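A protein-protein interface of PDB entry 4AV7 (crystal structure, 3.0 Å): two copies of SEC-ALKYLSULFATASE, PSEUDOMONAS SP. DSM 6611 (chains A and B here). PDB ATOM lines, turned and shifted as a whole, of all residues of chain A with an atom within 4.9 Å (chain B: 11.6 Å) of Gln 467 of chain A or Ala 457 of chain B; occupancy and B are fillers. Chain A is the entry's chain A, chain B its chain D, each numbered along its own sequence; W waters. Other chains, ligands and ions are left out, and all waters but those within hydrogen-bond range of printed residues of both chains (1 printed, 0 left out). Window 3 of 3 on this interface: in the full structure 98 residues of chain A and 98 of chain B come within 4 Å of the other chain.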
ATOM      1  N   ALA A 457     -32.997   2.153   1.805  1.00  0.00           N
ATOM      2  CA  ALA A 457     -32.865   1.360   0.578  1.00  0.00           C
ATOM      3  C   ALA A 457     -32.567  -0.105   0.851  1.00  0.00           C
ATOM      4  O   ALA A 457     -32.880  -0.970   0.032  1.00  0.00           O
ATOM      5  CB  ALA A 457     -31.806   1.957  -0.340  1.00  0.00           C
ATOM      6  N   MET A 458     -31.955  -0.371   1.998  1.00  0.00           N
ATOM      7  CA  MET A 458     -31.682  -1.740   2.419  1.00  0.00           C
ATOM      8  C   MET A 458     -32.800  -2.377   3.261  1.00  0.00           C
ATOM      9  O   MET A 458     -32.766  -3.588   3.510  1.00  0.00           O
ATOM     10  CB  MET A 458     -30.354  -1.799   3.141  1.00  0.00           C
ATOM     11  CG  MET A 458     -29.189  -1.624   2.197  1.00  0.00           C
ATOM     12  SD  MET A 458     -27.665  -1.409   3.118  1.00  0.00           S
ATOM     13  CE  MET A 458     -26.700  -0.445   1.962  1.00  0.00           C
ATOM     14  N   ALA A 463     -33.303  -4.634   9.260  1.00  0.00           N
ATOM     15  CA  ALA A 463     -32.799  -5.343   8.084  1.00  0.00           C
ATOM     16  C   ALA A 463     -31.285  -5.172   7.912  1.00  0.00           C
ATOM     17  O   ALA A 463     -30.589  -6.135   7.572  1.00  0.00           O
ATOM     18  CB  ALA A 463     -33.523  -4.901   6.822  1.00  0.00           C
ATOM     19  N   VAL A 464     -30.771  -3.959   8.137  1.00  0.00           N
ATOM     20  CA  VAL A 464     -29.332  -3.744   7.991  1.00  0.00           C
ATOM     21  C   VAL A 464     -28.546  -4.385   9.158  1.00  0.00           C
ATOM     22  O   VAL A 464     -27.457  -4.913   8.957  1.00  0.00           O
ATOM     23  CB  VAL A 464     -28.933  -2.258   7.719  1.00  0.00           C
ATOM     24  CG1 VAL A 464     -29.678  -1.676   6.527  1.00  0.00           C
ATOM     25  CG2 VAL A 464     -29.133  -1.376   8.936  1.00  0.00           C
ATOM     26  N   LEU A 465     -29.111  -4.372  10.363  1.00  0.00           N
ATOM     27  CA  LEU A 465     -28.491  -5.062  11.507  1.00  0.00           C
ATOM     28  C   LEU A 465     -28.404  -6.558  11.252  1.00  0.00           C
ATOM     29  O   LEU A 465     -27.433  -7.217  11.642  1.00  0.00           O
ATOM     30  CB  LEU A 465     -29.263  -4.793  12.791  1.00  0.00           C
ATOM     31  CG  LEU A 465     -29.033  -3.376  13.298  1.00  0.00           C
ATOM     32  CD1 LEU A 465     -30.253  -2.855  14.040  1.00  0.00           C
ATOM     33  CD2 LEU A 465     -27.790  -3.328  14.169  1.00  0.00           C
ATOM     34  N   LYS A 466     -29.419  -7.080  10.573  1.00  0.00           N
ATOM     35  CA  LYS A 466     -29.410  -8.464  10.154  1.00  0.00           C
ATOM     36  C   LYS A 466     -28.217  -8.671   9.237  1.00  0.00           C
ATOM     37  O   LYS A 466     -27.403  -9.570   9.464  1.00  0.00           O
ATOM     38  CB  LYS A 466     -30.715  -8.836   9.452  1.00  0.00           C
ATOM     39  CG  LYS A 466     -31.001 -10.326   9.506  1.00  0.00           C
ATOM     40  CD  LYS A 466     -32.312 -10.709   8.842  1.00  0.00           C
ATOM     41  CE  LYS A 466     -32.300 -12.204   8.535  1.00  0.00           C
ATOM     42  NZ  LYS A 466     -33.267 -12.563   7.457  1.00  0.00           N
ATOM     43  N   GLN A 467     -28.100  -7.803   8.233  1.00  0.00           N
ATOM     44  CA  GLN A 467     -27.012  -7.870   7.262  1.00  0.00           C
ATOM     45  C   GLN A 467     -25.654  -7.667   7.913  1.00  0.00           C
ATOM     46  O   GLN A 467     -24.661  -8.302   7.535  1.00  0.00           O
ATOM     47  CB  GLN A 467     -27.212  -6.829   6.189  1.00  0.00           C
ATOM     48  CG  GLN A 467     -28.352  -7.150   5.242  1.00  0.00           C
ATOM     49  CD  GLN A 467     -28.275  -6.314   3.983  1.00  0.00           C
ATOM     50  OE1 GLN A 467     -27.191  -6.167   3.391  1.00  0.00           O
ATOM     51  NE2 GLN A 467     -29.412  -5.752   3.562  1.00  0.00           N
ATOM     52  N   MET A 468     -25.621  -6.785   8.905  1.00  0.00           N
ATOM     53  CA  MET A 468     -24.414  -6.561   9.681  1.00  0.00           C
ATOM     54  C   MET A 468     -23.989  -7.832  10.362  1.00  0.00           C
ATOM     55  O   MET A 468     -22.819  -8.231  10.233  1.00  0.00           O
ATOM     56  CB  MET A 468     -24.624  -5.488  10.730  1.00  0.00           C
ATOM     57  CG  MET A 468     -24.119  -4.132  10.294  1.00  0.00           C
ATOM     58  SD  MET A 468     -24.018  -2.991  11.685  1.00  0.00           S
ATOM     59  CE  MET A 468     -25.580  -2.134  11.420  1.00  0.00           C
ATOM     60  N   ARG A 469     -24.954  -8.457  11.063  1.00  0.00           N
ATOM     61  CA  ARG A 469     -24.729  -9.699  11.819  1.00  0.00           C
ATOM     62  C   ARG A 469     -24.174 -10.783  10.915  1.00  0.00           C
ATOM     63  O   ARG A 469     -23.129 -11.362  11.205  1.00  0.00           O
ATOM     64  CB  ARG A 469     -25.992 -10.152  12.552  1.00  0.00           C
ATOM     65  CG  ARG A 469     -26.124  -9.474  13.899  1.00  0.00           C
ATOM     66  CD  ARG A 469     -27.233 -10.010  14.790  1.00  0.00           C
ATOM     67  NE  ARG A 469     -27.438  -9.077  15.900  1.00  0.00           N
ATOM     68  CZ  ARG A 469     -28.464  -8.232  15.986  1.00  0.00           C
ATOM     69  NH1 ARG A 469     -29.413  -8.218  15.046  1.00  0.00           N
ATOM     70  NH2 ARG A 469     -28.547  -7.396  17.015  1.00  0.00           N
ATOM     71  N   ALA A 470     -24.850 -10.992   9.785  1.00  0.00           N
ATOM     72  CA  ALA A 470     -24.426 -11.956   8.763  1.00  0.00           C
ATOM     73  C   ALA A 470     -22.976 -11.690   8.270  1.00  0.00           C
ATOM     74  O   ALA A 470     -22.205 -12.628   8.037  1.00  0.00           O
ATOM     75  CB  ALA A 470     -25.426 -11.968   7.607  1.00  0.00           C
ATOM     76  N   ALA A 471     -22.614 -10.411   8.154  1.00  0.00           N
ATOM     77  CA  ALA A 471     -21.291 -10.024   7.706  1.00  0.00           C
ATOM     78  C   ALA A 471     -20.223 -10.311   8.755  1.00  0.00           C
ATOM     79  O   ALA A 471     -19.128 -10.756   8.402  1.00  0.00           O
ATOM     80  CB  ALA A 471     -21.275  -8.556   7.317  1.00  0.00           C
ATOM     81  N   TRP A 479     -16.951  -5.135   5.375  1.00  0.00           N
ATOM     82  CA  TRP A 479     -18.251  -4.751   4.845  1.00  0.00           C
ATOM     83  C   TRP A 479     -19.131  -4.315   5.960  1.00  0.00           C
ATOM     84  O   TRP A 479     -19.875  -3.332   5.833  1.00  0.00           O
ATOM     85  CB  TRP A 479     -18.896  -5.853   4.018  1.00  0.00           C
ATOM     86  CG  TRP A 479     -20.258  -5.478   3.490  1.00  0.00           C
ATOM     87  CD1 TRP A 479     -21.461  -6.068   3.807  1.00  0.00           C
ATOM     88  CD2 TRP A 479     -20.608  -4.386   2.554  1.00  0.00           C
ATOM     89  NE1 TRP A 479     -22.493  -5.454   3.150  1.00  0.00           N
ATOM     90  CE2 TRP A 479     -22.054  -4.445   2.385  1.00  0.00           C
ATOM     91  CE3 TRP A 479     -19.886  -3.420   1.851  1.00  0.00           C
ATOM     92  CZ2 TRP A 479     -22.737  -3.576   1.553  1.00  0.00           C
ATOM     93  CZ3 TRP A 479     -20.587  -2.540   1.018  1.00  0.00           C
ATOM     94  CH2 TRP A 479     -21.979  -2.613   0.877  1.00  0.00           C
ATOM     95  N   LEU A 483     -21.540  -0.840   6.262  1.00  0.00           N
ATOM     96  CA  LEU A 483     -22.948  -1.015   6.540  1.00  0.00           C
ATOM     97  C   LEU A 483     -23.325  -0.242   7.814  1.00  0.00           C
ATOM     98  O   LEU A 483     -24.258   0.577   7.829  1.00  0.00           O
ATOM     99  CB  LEU A 483     -23.156  -2.519   6.740  1.00  0.00           C
ATOM    100  CG  LEU A 483     -24.288  -3.272   6.043  1.00  0.00           C
ATOM    101  CD1 LEU A 483     -24.438  -2.938   4.567  1.00  0.00           C
ATOM    102  CD2 LEU A 483     -24.029  -4.761   6.204  1.00  0.00           C
ATOM    103  N   PHE B 445     -14.042  -0.079  -0.740  1.00  0.00           N
ATOM    104  CA  PHE B 445     -14.038  -1.091  -1.774  1.00  0.00           C
ATOM    105  C   PHE B 445     -13.995  -0.402  -3.131  1.00  0.00           C
ATOM    106  O   PHE B 445     -14.524   0.700  -3.273  1.00  0.00           O
ATOM    107  CB  PHE B 445     -15.317  -1.921  -1.680  1.00  0.00           C
ATOM    108  CG  PHE B 445     -15.314  -2.950  -0.585  1.00  0.00           C
ATOM    109  CD1 PHE B 445     -14.719  -4.184  -0.769  1.00  0.00           C
ATOM    110  CD2 PHE B 445     -15.954  -2.701   0.607  1.00  0.00           C
ATOM    111  CE1 PHE B 445     -14.732  -5.137   0.235  1.00  0.00           C
ATOM    112  CE2 PHE B 445     -15.975  -3.648   1.619  1.00  0.00           C
ATOM    113  CZ  PHE B 445     -15.363  -4.867   1.435  1.00  0.00           C
ATOM    114  N   VAL B 448     -16.541  -1.767  -8.549  1.00  0.00           N
ATOM    115  CA  VAL B 448     -17.159  -3.070  -8.872  1.00  0.00           C
ATOM    116  C   VAL B 448     -17.546  -3.878  -7.616  1.00  0.00           C
ATOM    117  O   VAL B 448     -18.696  -4.299  -7.464  1.00  0.00           O
ATOM    118  CB  VAL B 448     -16.299  -3.927  -9.799  1.00  0.00           C
ATOM    119  CG1 VAL B 448     -17.118  -5.122 -10.248  1.00  0.00           C
ATOM    120  CG2 VAL B 448     -15.873  -3.114 -11.000  1.00  0.00           C
ATOM    121  N   GLU B 449     -16.572  -4.075  -6.729  1.00  0.00           N
ATOM    122  CA  GLU B 449     -16.779  -4.746  -5.452  1.00  0.00           C
ATOM    123  C   GLU B 449     -17.905  -4.123  -4.631  1.00  0.00           C
ATOM    124  O   GLU B 449     -18.818  -4.813  -4.187  1.00  0.00           O
ATOM    125  CB  GLU B 449     -15.481  -4.730  -4.654  1.00  0.00           C
ATOM    126  CG  GLU B 449     -14.711  -6.017  -4.762  1.00  0.00           C
ATOM    127  CD  GLU B 449     -15.442  -7.131  -4.039  1.00  0.00           C
ATOM    128  OE1 GLU B 449     -15.558  -7.039  -2.793  1.00  0.00           O
ATOM    129  OE2 GLU B 449     -15.915  -8.083  -4.716  1.00  0.00           O
ATOM    130  N   ALA B 450     -17.836  -2.815  -4.441  1.00  0.00           N
ATOM    131  CA  ALA B 450     -18.799  -2.105  -3.627  1.00  0.00           C
ATOM    132  C   ALA B 450     -20.137  -2.070  -4.306  1.00  0.00           C
ATOM    133  O   ALA B 450     -21.147  -2.068  -3.625  1.00  0.00           O
ATOM    134  CB  ALA B 450     -18.335  -0.691  -3.375  1.00  0.00           C
ATOM    135  N   GLY B 451     -20.145  -2.030  -5.643  1.00  0.00           N
ATOM    136  CA  GLY B 451     -21.403  -2.065  -6.409  1.00  0.00           C
ATOM    137  C   GLY B 451     -22.187  -3.355  -6.154  1.00  0.00           C
ATOM    138  O   GLY B 451     -23.320  -3.326  -5.645  1.00  0.00           O
ATOM    139  N   LYS B 452     -21.563  -4.484  -6.498  1.00  0.00           N
ATOM    140  CA  LYS B 452     -22.087  -5.825  -6.234  1.00  0.00           C
ATOM    141  C   LYS B 452     -22.669  -6.029  -4.819  1.00  0.00           C
ATOM    142  O   LYS B 452     -23.716  -6.651  -4.678  1.00  0.00           O
ATOM    143  CB  LYS B 452     -21.003  -6.861  -6.505  1.00  0.00           C
ATOM    144  CG  LYS B 452     -20.729  -7.046  -7.985  1.00  0.00           C
ATOM    145  CD  LYS B 452     -19.686  -8.130  -8.228  1.00  0.00           C
ATOM    146  CE  LYS B 452     -19.607  -8.522  -9.690  1.00  0.00           C
ATOM    147  NZ  LYS B 452     -18.727  -9.717  -9.825  1.00  0.00           N
ATOM    148  N   ARG B 453     -21.984  -5.500  -3.800  1.00  0.00           N
ATOM    149  CA  ARG B 453     -22.366  -5.626  -2.388  1.00  0.00           C
ATOM    150  C   ARG B 453     -23.536  -4.741  -1.976  1.00  0.00           C
ATOM    151  O   ARG B 453     -24.329  -5.109  -1.128  1.00  0.00           O
ATOM    152  CB  ARG B 453     -21.173  -5.264  -1.506  1.00  0.00           C
ATOM    153  CG  ARG B 453     -20.116  -6.343  -1.456  1.00  0.00           C
ATOM    154  CD  ARG B 453     -18.832  -5.796  -0.892  1.00  0.00           C
ATOM    155  NE  ARG B 453     -17.780  -6.804  -0.917  1.00  0.00           N
ATOM    156  CZ  ARG B 453     -17.529  -7.617   0.101  1.00  0.00           C
ATOM    157  NH1 ARG B 453     -18.272  -7.545   1.205  1.00  0.00           N
ATOM    158  NH2 ARG B 453     -16.550  -8.505   0.014  1.00  0.00           N
ATOM    159  N   TYR B 454     -23.608  -3.554  -2.555  1.00  0.00           N
ATOM    160  CA  TYR B 454     -24.710  -2.645  -2.334  1.00  0.00           C
ATOM    161  C   TYR B 454     -25.981  -3.147  -3.045  1.00  0.00           C
ATOM    162  O   TYR B 454     -27.088  -3.069  -2.506  1.00  0.00           O
ATOM    163  CB  TYR B 454     -24.333  -1.236  -2.824  1.00  0.00           C
ATOM    164  CG  TYR B 454     -23.636  -0.387  -1.780  1.00  0.00           C
ATOM    165  CD1 TYR B 454     -24.283  -0.047  -0.598  1.00  0.00           C
ATOM    166  CD2 TYR B 454     -22.342   0.084  -1.964  1.00  0.00           C
ATOM    167  CE1 TYR B 454     -23.670   0.728   0.370  1.00  0.00           C
ATOM    168  CE2 TYR B 454     -21.728   0.857  -0.985  1.00  0.00           C
ATOM    169  CZ  TYR B 454     -22.406   1.178   0.169  1.00  0.00           C
ATOM    170  OH  TYR B 454     -21.841   1.942   1.157  1.00  0.00           O
ATOM    171  N   VAL B 455     -25.828  -3.666  -4.255  1.00  0.00           N
ATOM    172  CA  VAL B 455     -26.982  -4.201  -4.969  1.00  0.00           C
ATOM    173  C   VAL B 455     -27.640  -5.370  -4.185  1.00  0.00           C
ATOM    174  O   VAL B 455     -28.819  -5.307  -3.863  1.00  0.00           O
ATOM    175  CB  VAL B 455     -26.631  -4.544  -6.439  1.00  0.00           C
ATOM    176  CG1 VAL B 455     -27.806  -5.219  -7.117  1.00  0.00           C
ATOM    177  CG2 VAL B 455     -26.277  -3.277  -7.209  1.00  0.00           C
ATOM    178  N   GLU B 456     -26.862  -6.408  -3.873  1.00  0.00           N
ATOM    179  CA  GLU B 456     -27.238  -7.451  -2.928  1.00  0.00           C
ATOM    180  C   GLU B 456     -27.924  -6.910  -1.677  1.00  0.00           C
ATOM    181  O   GLU B 456     -28.957  -7.429  -1.262  1.00  0.00           O
ATOM    182  CB  GLU B 456     -25.982  -8.179  -2.474  1.00  0.00           C
ATOM    183  CG  GLU B 456     -26.209  -9.270  -1.417  1.00  0.00           C
ATOM    184  CD  GLU B 456     -24.957 -10.082  -1.206  1.00  0.00           C
ATOM    185  OE1 GLU B 456     -24.257 -10.403  -2.203  1.00  0.00           O
ATOM    186  OE2 GLU B 456     -24.671 -10.404  -0.033  1.00  0.00           O
ATOM    187  N   ALA B 457     -27.341  -5.888  -1.066  1.00  0.00           N
ATOM    188  CA  ALA B 457     -27.837  -5.370   0.199  1.00  0.00           C
ATOM    189  C   ALA B 457     -29.221  -4.776   0.114  1.00  0.00           C
ATOM    190  O   ALA B 457     -29.862  -4.588   1.151  1.00  0.00           O
ATOM    191  CB  ALA B 457     -26.886  -4.324   0.750  1.00  0.00           C
ATOM    192  N   MET B 458     -29.651  -4.454  -1.109  1.00  0.00           N
ATOM    193  CA  MET B 458     -30.879  -3.706  -1.351  1.00  0.00           C
ATOM    194  C   MET B 458     -31.912  -4.616  -2.004  1.00  0.00           C
ATOM    195  O   MET B 458     -33.086  -4.244  -2.141  1.00  0.00           O
ATOM    196  CB  MET B 458     -30.610  -2.479  -2.225  1.00  0.00           C
ATOM    197  CG  MET B 458     -29.781  -1.377  -1.567  1.00  0.00           C
ATOM    198  SD  MET B 458     -29.331  -0.012  -2.679  1.00  0.00           S
ATOM    199  CE  MET B 458     -27.789   0.494  -1.954  1.00  0.00           C
ATOM    200  N   GLY B 459     -31.469  -5.810  -2.398  1.00  0.00           N
ATOM    201  CA  GLY B 459     -32.370  -6.865  -2.854  1.00  0.00           C
ATOM    202  C   GLY B 459     -32.148  -7.345  -4.279  1.00  0.00           C
ATOM    203  O   GLY B 459     -32.897  -8.182  -4.793  1.00  0.00           O
ATOM    204  N   GLY B 460     -31.123  -6.818  -4.930  1.00  0.00           N
ATOM    205  CA  GLY B 460     -30.739  -7.332  -6.240  1.00  0.00           C
ATOM    206  C   GLY B 460     -31.111  -6.345  -7.314  1.00  0.00           C
ATOM    207  O   GLY B 460     -31.719  -5.293  -7.035  1.00  0.00           O
ATOM    208  N   ALA B 461     -30.743  -6.686  -8.544  1.00  0.00           N
ATOM    209  CA  ALA B 461     -30.924  -5.788  -9.673  1.00  0.00           C
ATOM    210  C   ALA B 461     -32.340  -5.193  -9.722  1.00  0.00           C
ATOM    211  O   ALA B 461     -32.514  -3.975  -9.578  1.00  0.00           O
ATOM    212  CB  ALA B 461     -30.559  -6.486 -10.978  1.00  0.00           C
ATOM    213  N   ASP B 462     -33.352  -6.047  -9.875  1.00  0.00           N
ATOM    214  CA  ASP B 462     -34.731  -5.563 -10.045  1.00  0.00           C
ATOM    215  C   ASP B 462     -35.217  -4.669  -8.877  1.00  0.00           C
ATOM    216  O   ASP B 462     -35.970  -3.710  -9.091  1.00  0.00           O
ATOM    217  CB  ASP B 462     -35.688  -6.739 -10.308  1.00  0.00           C
ATOM    218  CG  ASP B 462     -35.227  -7.621 -11.475  1.00  0.00           C
ATOM    219  OD1 ASP B 462     -34.162  -7.344 -12.054  1.00  0.00           O
ATOM    220  OD2 ASP B 462     -35.918  -8.601 -11.821  1.00  0.00           O
ATOM    221  N   ALA B 463     -34.760  -4.966  -7.657  1.00  0.00           N
ATOM    222  CA  ALA B 463     -35.133  -4.179  -6.471  1.00  0.00           C
ATOM    223  C   ALA B 463     -34.574  -2.769  -6.519  1.00  0.00           C
ATOM    224  O   ALA B 463     -35.264  -1.815  -6.135  1.00  0.00           O
ATOM    225  CB  ALA B 463     -34.695  -4.874  -5.191  1.00  0.00           C
ATOM    226  N   VAL B 464     -33.328  -2.641  -6.980  1.00  0.00           N
ATOM    227  CA  VAL B 464     -32.715  -1.324  -7.093  1.00  0.00           C
ATOM    228  C   VAL B 464     -33.286  -0.577  -8.298  1.00  0.00           C
ATOM    229  O   VAL B 464     -33.567   0.621  -8.205  1.00  0.00           O
ATOM    230  CB  VAL B 464     -31.162  -1.359  -7.093  1.00  0.00           C
ATOM    231  CG1 VAL B 464     -30.636  -2.149  -5.899  1.00  0.00           C
ATOM    232  CG2 VAL B 464     -30.601  -1.934  -8.381  1.00  0.00           C
ATOM    233  N   LEU B 465     -33.496  -1.297  -9.405  1.00  0.00           N
ATOM    234  CA  LEU B 465     -34.126  -0.725 -10.594  1.00  0.00           C
ATOM    235  C   LEU B 465     -35.420  -0.029 -10.217  1.00  0.00           C
ATOM    236  O   LEU B 465     -35.636   1.135 -10.569  1.00  0.00           O
ATOM    237  CB  LEU B 465     -34.411  -1.803 -11.629  1.00  0.00           C
ATOM    238  CG  LEU B 465     -33.248  -2.212 -12.521  1.00  0.00           C
ATOM    239  CD1 LEU B 465     -33.568  -3.534 -13.209  1.00  0.00           C
ATOM    240  CD2 LEU B 465     -32.934  -1.129 -13.540  1.00  0.00           C
ATOM    241  N   GLN B 467     -36.235   0.959  -7.220  1.00  0.00           N
ATOM    242  CA  GLN B 467     -35.880   2.104  -6.381  1.00  0.00           C
ATOM    243  C   GLN B 467     -35.395   3.279  -7.234  1.00  0.00           C
ATOM    244  O   GLN B 467     -35.614   4.456  -6.894  1.00  0.00           O
ATOM    245  CB  GLN B 467     -34.799   1.726  -5.371  1.00  0.00           C
ATOM    246  CG  GLN B 467     -35.266   0.853  -4.218  1.00  0.00           C
ATOM    247  CD  GLN B 467     -34.224   0.737  -3.110  1.00  0.00           C
ATOM    248  OE1 GLN B 467     -33.766   1.748  -2.569  1.00  0.00           O
ATOM    249  NE2 GLN B 467     -33.854  -0.497  -2.760  1.00  0.00           N
ATOM    250  N   TRP B 479     -29.876  10.883  -6.173  1.00  0.00           N
ATOM    251  CA  TRP B 479     -29.836   9.539  -5.588  1.00  0.00           C
ATOM    252  C   TRP B 479     -29.889   8.463  -6.649  1.00  0.00           C
ATOM    253  O   TRP B 479     -29.221   7.437  -6.524  1.00  0.00           O
ATOM    254  CB  TRP B 479     -30.950   9.375  -4.559  1.00  0.00           C
ATOM    255  CG  TRP B 479     -30.994   8.026  -3.879  1.00  0.00           C
ATOM    256  CD1 TRP B 479     -31.952   7.025  -4.037  1.00  0.00           C
ATOM    257  CD2 TRP B 479     -30.036   7.480  -2.910  1.00  0.00           C
ATOM    258  NE1 TRP B 479     -31.660   5.933  -3.261  1.00  0.00           N
ATOM    259  CE2 TRP B 479     -30.523   6.138  -2.560  1.00  0.00           C
ATOM    260  CE3 TRP B 479     -28.856   7.939  -2.334  1.00  0.00           C
ATOM    261  CZ2 TRP B 479     -29.848   5.323  -1.653  1.00  0.00           C
ATOM    262  CZ3 TRP B 479     -28.183   7.102  -1.426  1.00  0.00           C
ATOM    263  CH2 TRP B 479     -28.670   5.832  -1.092  1.00  0.00           C
ATOM    264  N   LEU B 483     -27.515   5.191  -6.950  1.00  0.00           N
ATOM    265  CA  LEU B 483     -28.133   3.884  -7.047  1.00  0.00           C
ATOM    266  C   LEU B 483     -27.745   3.160  -8.319  1.00  0.00           C
ATOM    267  O   LEU B 483     -27.402   1.979  -8.306  1.00  0.00           O
ATOM    268  CB  LEU B 483     -29.637   4.099  -7.063  1.00  0.00           C
ATOM    269  CG  LEU B 483     -30.490   3.311  -6.101  1.00  0.00           C
ATOM    270  CD1 LEU B 483     -29.918   3.373  -4.700  1.00  0.00           C
ATOM    271  CD2 LEU B 483     -31.851   3.968  -6.143  1.00  0.00           C
ATOM    272  N   HIS B 486     -23.784   1.842  -8.668  1.00  0.00           N
ATOM    273  CA  HIS B 486     -23.534   0.539  -8.094  1.00  0.00           C
ATOM    274  C   HIS B 486     -24.017  -0.549  -8.992  1.00  0.00           C
ATOM    275  O   HIS B 486     -23.334  -1.559  -9.165  1.00  0.00           O
ATOM    276  CB  HIS B 486     -24.254   0.417  -6.780  1.00  0.00           C
ATOM    277  CG  HIS B 486     -23.743   1.346  -5.733  1.00  0.00           C
ATOM    278  ND1 HIS B 486     -22.465   1.338  -5.333  1.00  0.00           N
ATOM    279  CD2 HIS B 486     -24.388   2.303  -4.974  1.00  0.00           C
ATOM    280  CE1 HIS B 486     -22.291   2.250  -4.383  1.00  0.00           C
ATOM    281  NE2 HIS B 486     -23.470   2.841  -4.158  1.00  0.00           N
ATOM    282  N   LEU B 487     -25.196  -0.363  -9.582  1.00  0.00           N
ATOM    283  CA  LEU B 487     -25.747  -1.406 -10.417  1.00  0.00           C
ATOM    284  C   LEU B 487     -24.950  -1.611 -11.706  1.00  0.00           C
ATOM    285  O   LEU B 487     -24.709  -2.762 -12.115  1.00  0.00           O
ATOM    286  CB  LEU B 487     -27.229  -1.156 -10.714  1.00  0.00           C
ATOM    287  CG  LEU B 487     -27.891  -2.323 -11.454  1.00  0.00           C
ATOM    288  CD1 LEU B 487     -27.597  -3.668 -10.780  1.00  0.00           C
ATOM    289  CD2 LEU B 487     -29.381  -2.069 -11.584  1.00  0.00           C
ATOM    290  N   ALA B 490     -21.810  -3.225 -10.837  1.00  0.00           N
ATOM    291  CA  ALA B 490     -22.027  -4.639 -10.501  1.00  0.00           C
ATOM    292  C   ALA B 490     -22.351  -5.456 -11.752  1.00  0.00           C
ATOM    293  O   ALA B 490     -21.804  -6.537 -11.940  1.00  0.00           O
ATOM    294  CB  ALA B 490     -23.113  -4.792  -9.458  1.00  0.00           C
HETATM  295  O   HOH W   1     -24.062  -7.285   1.367  1.00  0.00           O
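The backbone carbonyl oxygen of Ala 457 of chain A sits at hydrogen-bond distance from the side-chain amide nitrogen of Gln 467 of chain B (3.0 Å).
The backbone carbonyl oxygen of Ala 457 of chain B lies within hydrogen-bond range of the side-chain amide nitrogen of Gln 467 of chain A, at 2.7 Å.
NE of Arg 453 of chain B is in salt-bridge range of OE1 of Glu 449 of chain B (2.9 Å).
Among the printed residues, pairs that only touch across the chains: Ala 457 of chain A with Met 458 of chain B, Met 458 of chain A with Tyr 454 of chain B, Met 458 of chain A with Ala 457 of chain B, Met 458 of chain A with Met 458 of chain B, Trp 479 of chain A with Phe 445 of chain B, Trp 479 of chain A with Arg 453 of chain B and Trp 479 of chain A with Tyr 454 of chain B.
Gln 467 of chain A touches one residue of chain B.
Of chain A, only Met 458 and Gln 467 come within 4 Å of Ala 457 of chain B.
Ala 457 of chain A touches just these residues of chain B: Met 458 and Gln 467.
Printed residues of chain B within 4 Å of Met 458 of chain A: Tyr 454, Ala 457 and Met 458.
No residue of chain B comes within 4 Å of Ala 463 of chain A.
Val 464 of chain A touches none of the printed residues of chain B.
No residue of chain B comes within 4 Å of Lys 466 of chain A.
Met 468 of chain A touches none of the printed residues of chain B.
Ala 470 of chain A touches none of the printed residues of chain B.
Printed residues of chain B within 4 Å of Trp 479 of chain A: Phe 445, Arg 453 and Tyr 454.
Printed residues of chain A within 4 Å of Phe 445 of chain B: Trp 479 (3.9 Å).
Of the printed residues of chain A, Gln 467 of chain B touches Ala 457.
The nearest residue of chain A that does not touch Ala 457 of chain B is Trp 479 of chain A (4.3 Å).
Printed residues of chain A that touch a printed residue of chain B: Ala 457, Met 458, Gln 467 and Trp 479.
Hydrophobic or aromatic side chains of chain A within 4 Å of the printed part of chain B: Ala 457, Met 458 and Trp 479.
Hydrophobic or aromatic side chains of chain B that line the printed part of chain A: Phe 445, Tyr 454, Ala 457 and Met 458.
Among the printed residues, 9 pairs touch across the chains.
Ala 457 of chain A touches Met 458 of chain B, and with the chains exchanged Met 458 of chain A touches Ala 457 of chain B.
Ala 457 of chain A touches Gln 467 of chain B, and with the chains exchanged Gln 467 of chain A touches Ala 457 of chain B.
Met 458 of chain B touches its own counterpart, Met 458 of chain A.
Of the 9 pairs that touch across the chains among the printed residues, 5 have their exchanged pair printed and touching as well.
Water W1 lies within hydrogen-bond range of NE1 of Trp 479 of chain A, O of Arg 453 of chain B and OE2 of Glu 456 of chain B.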
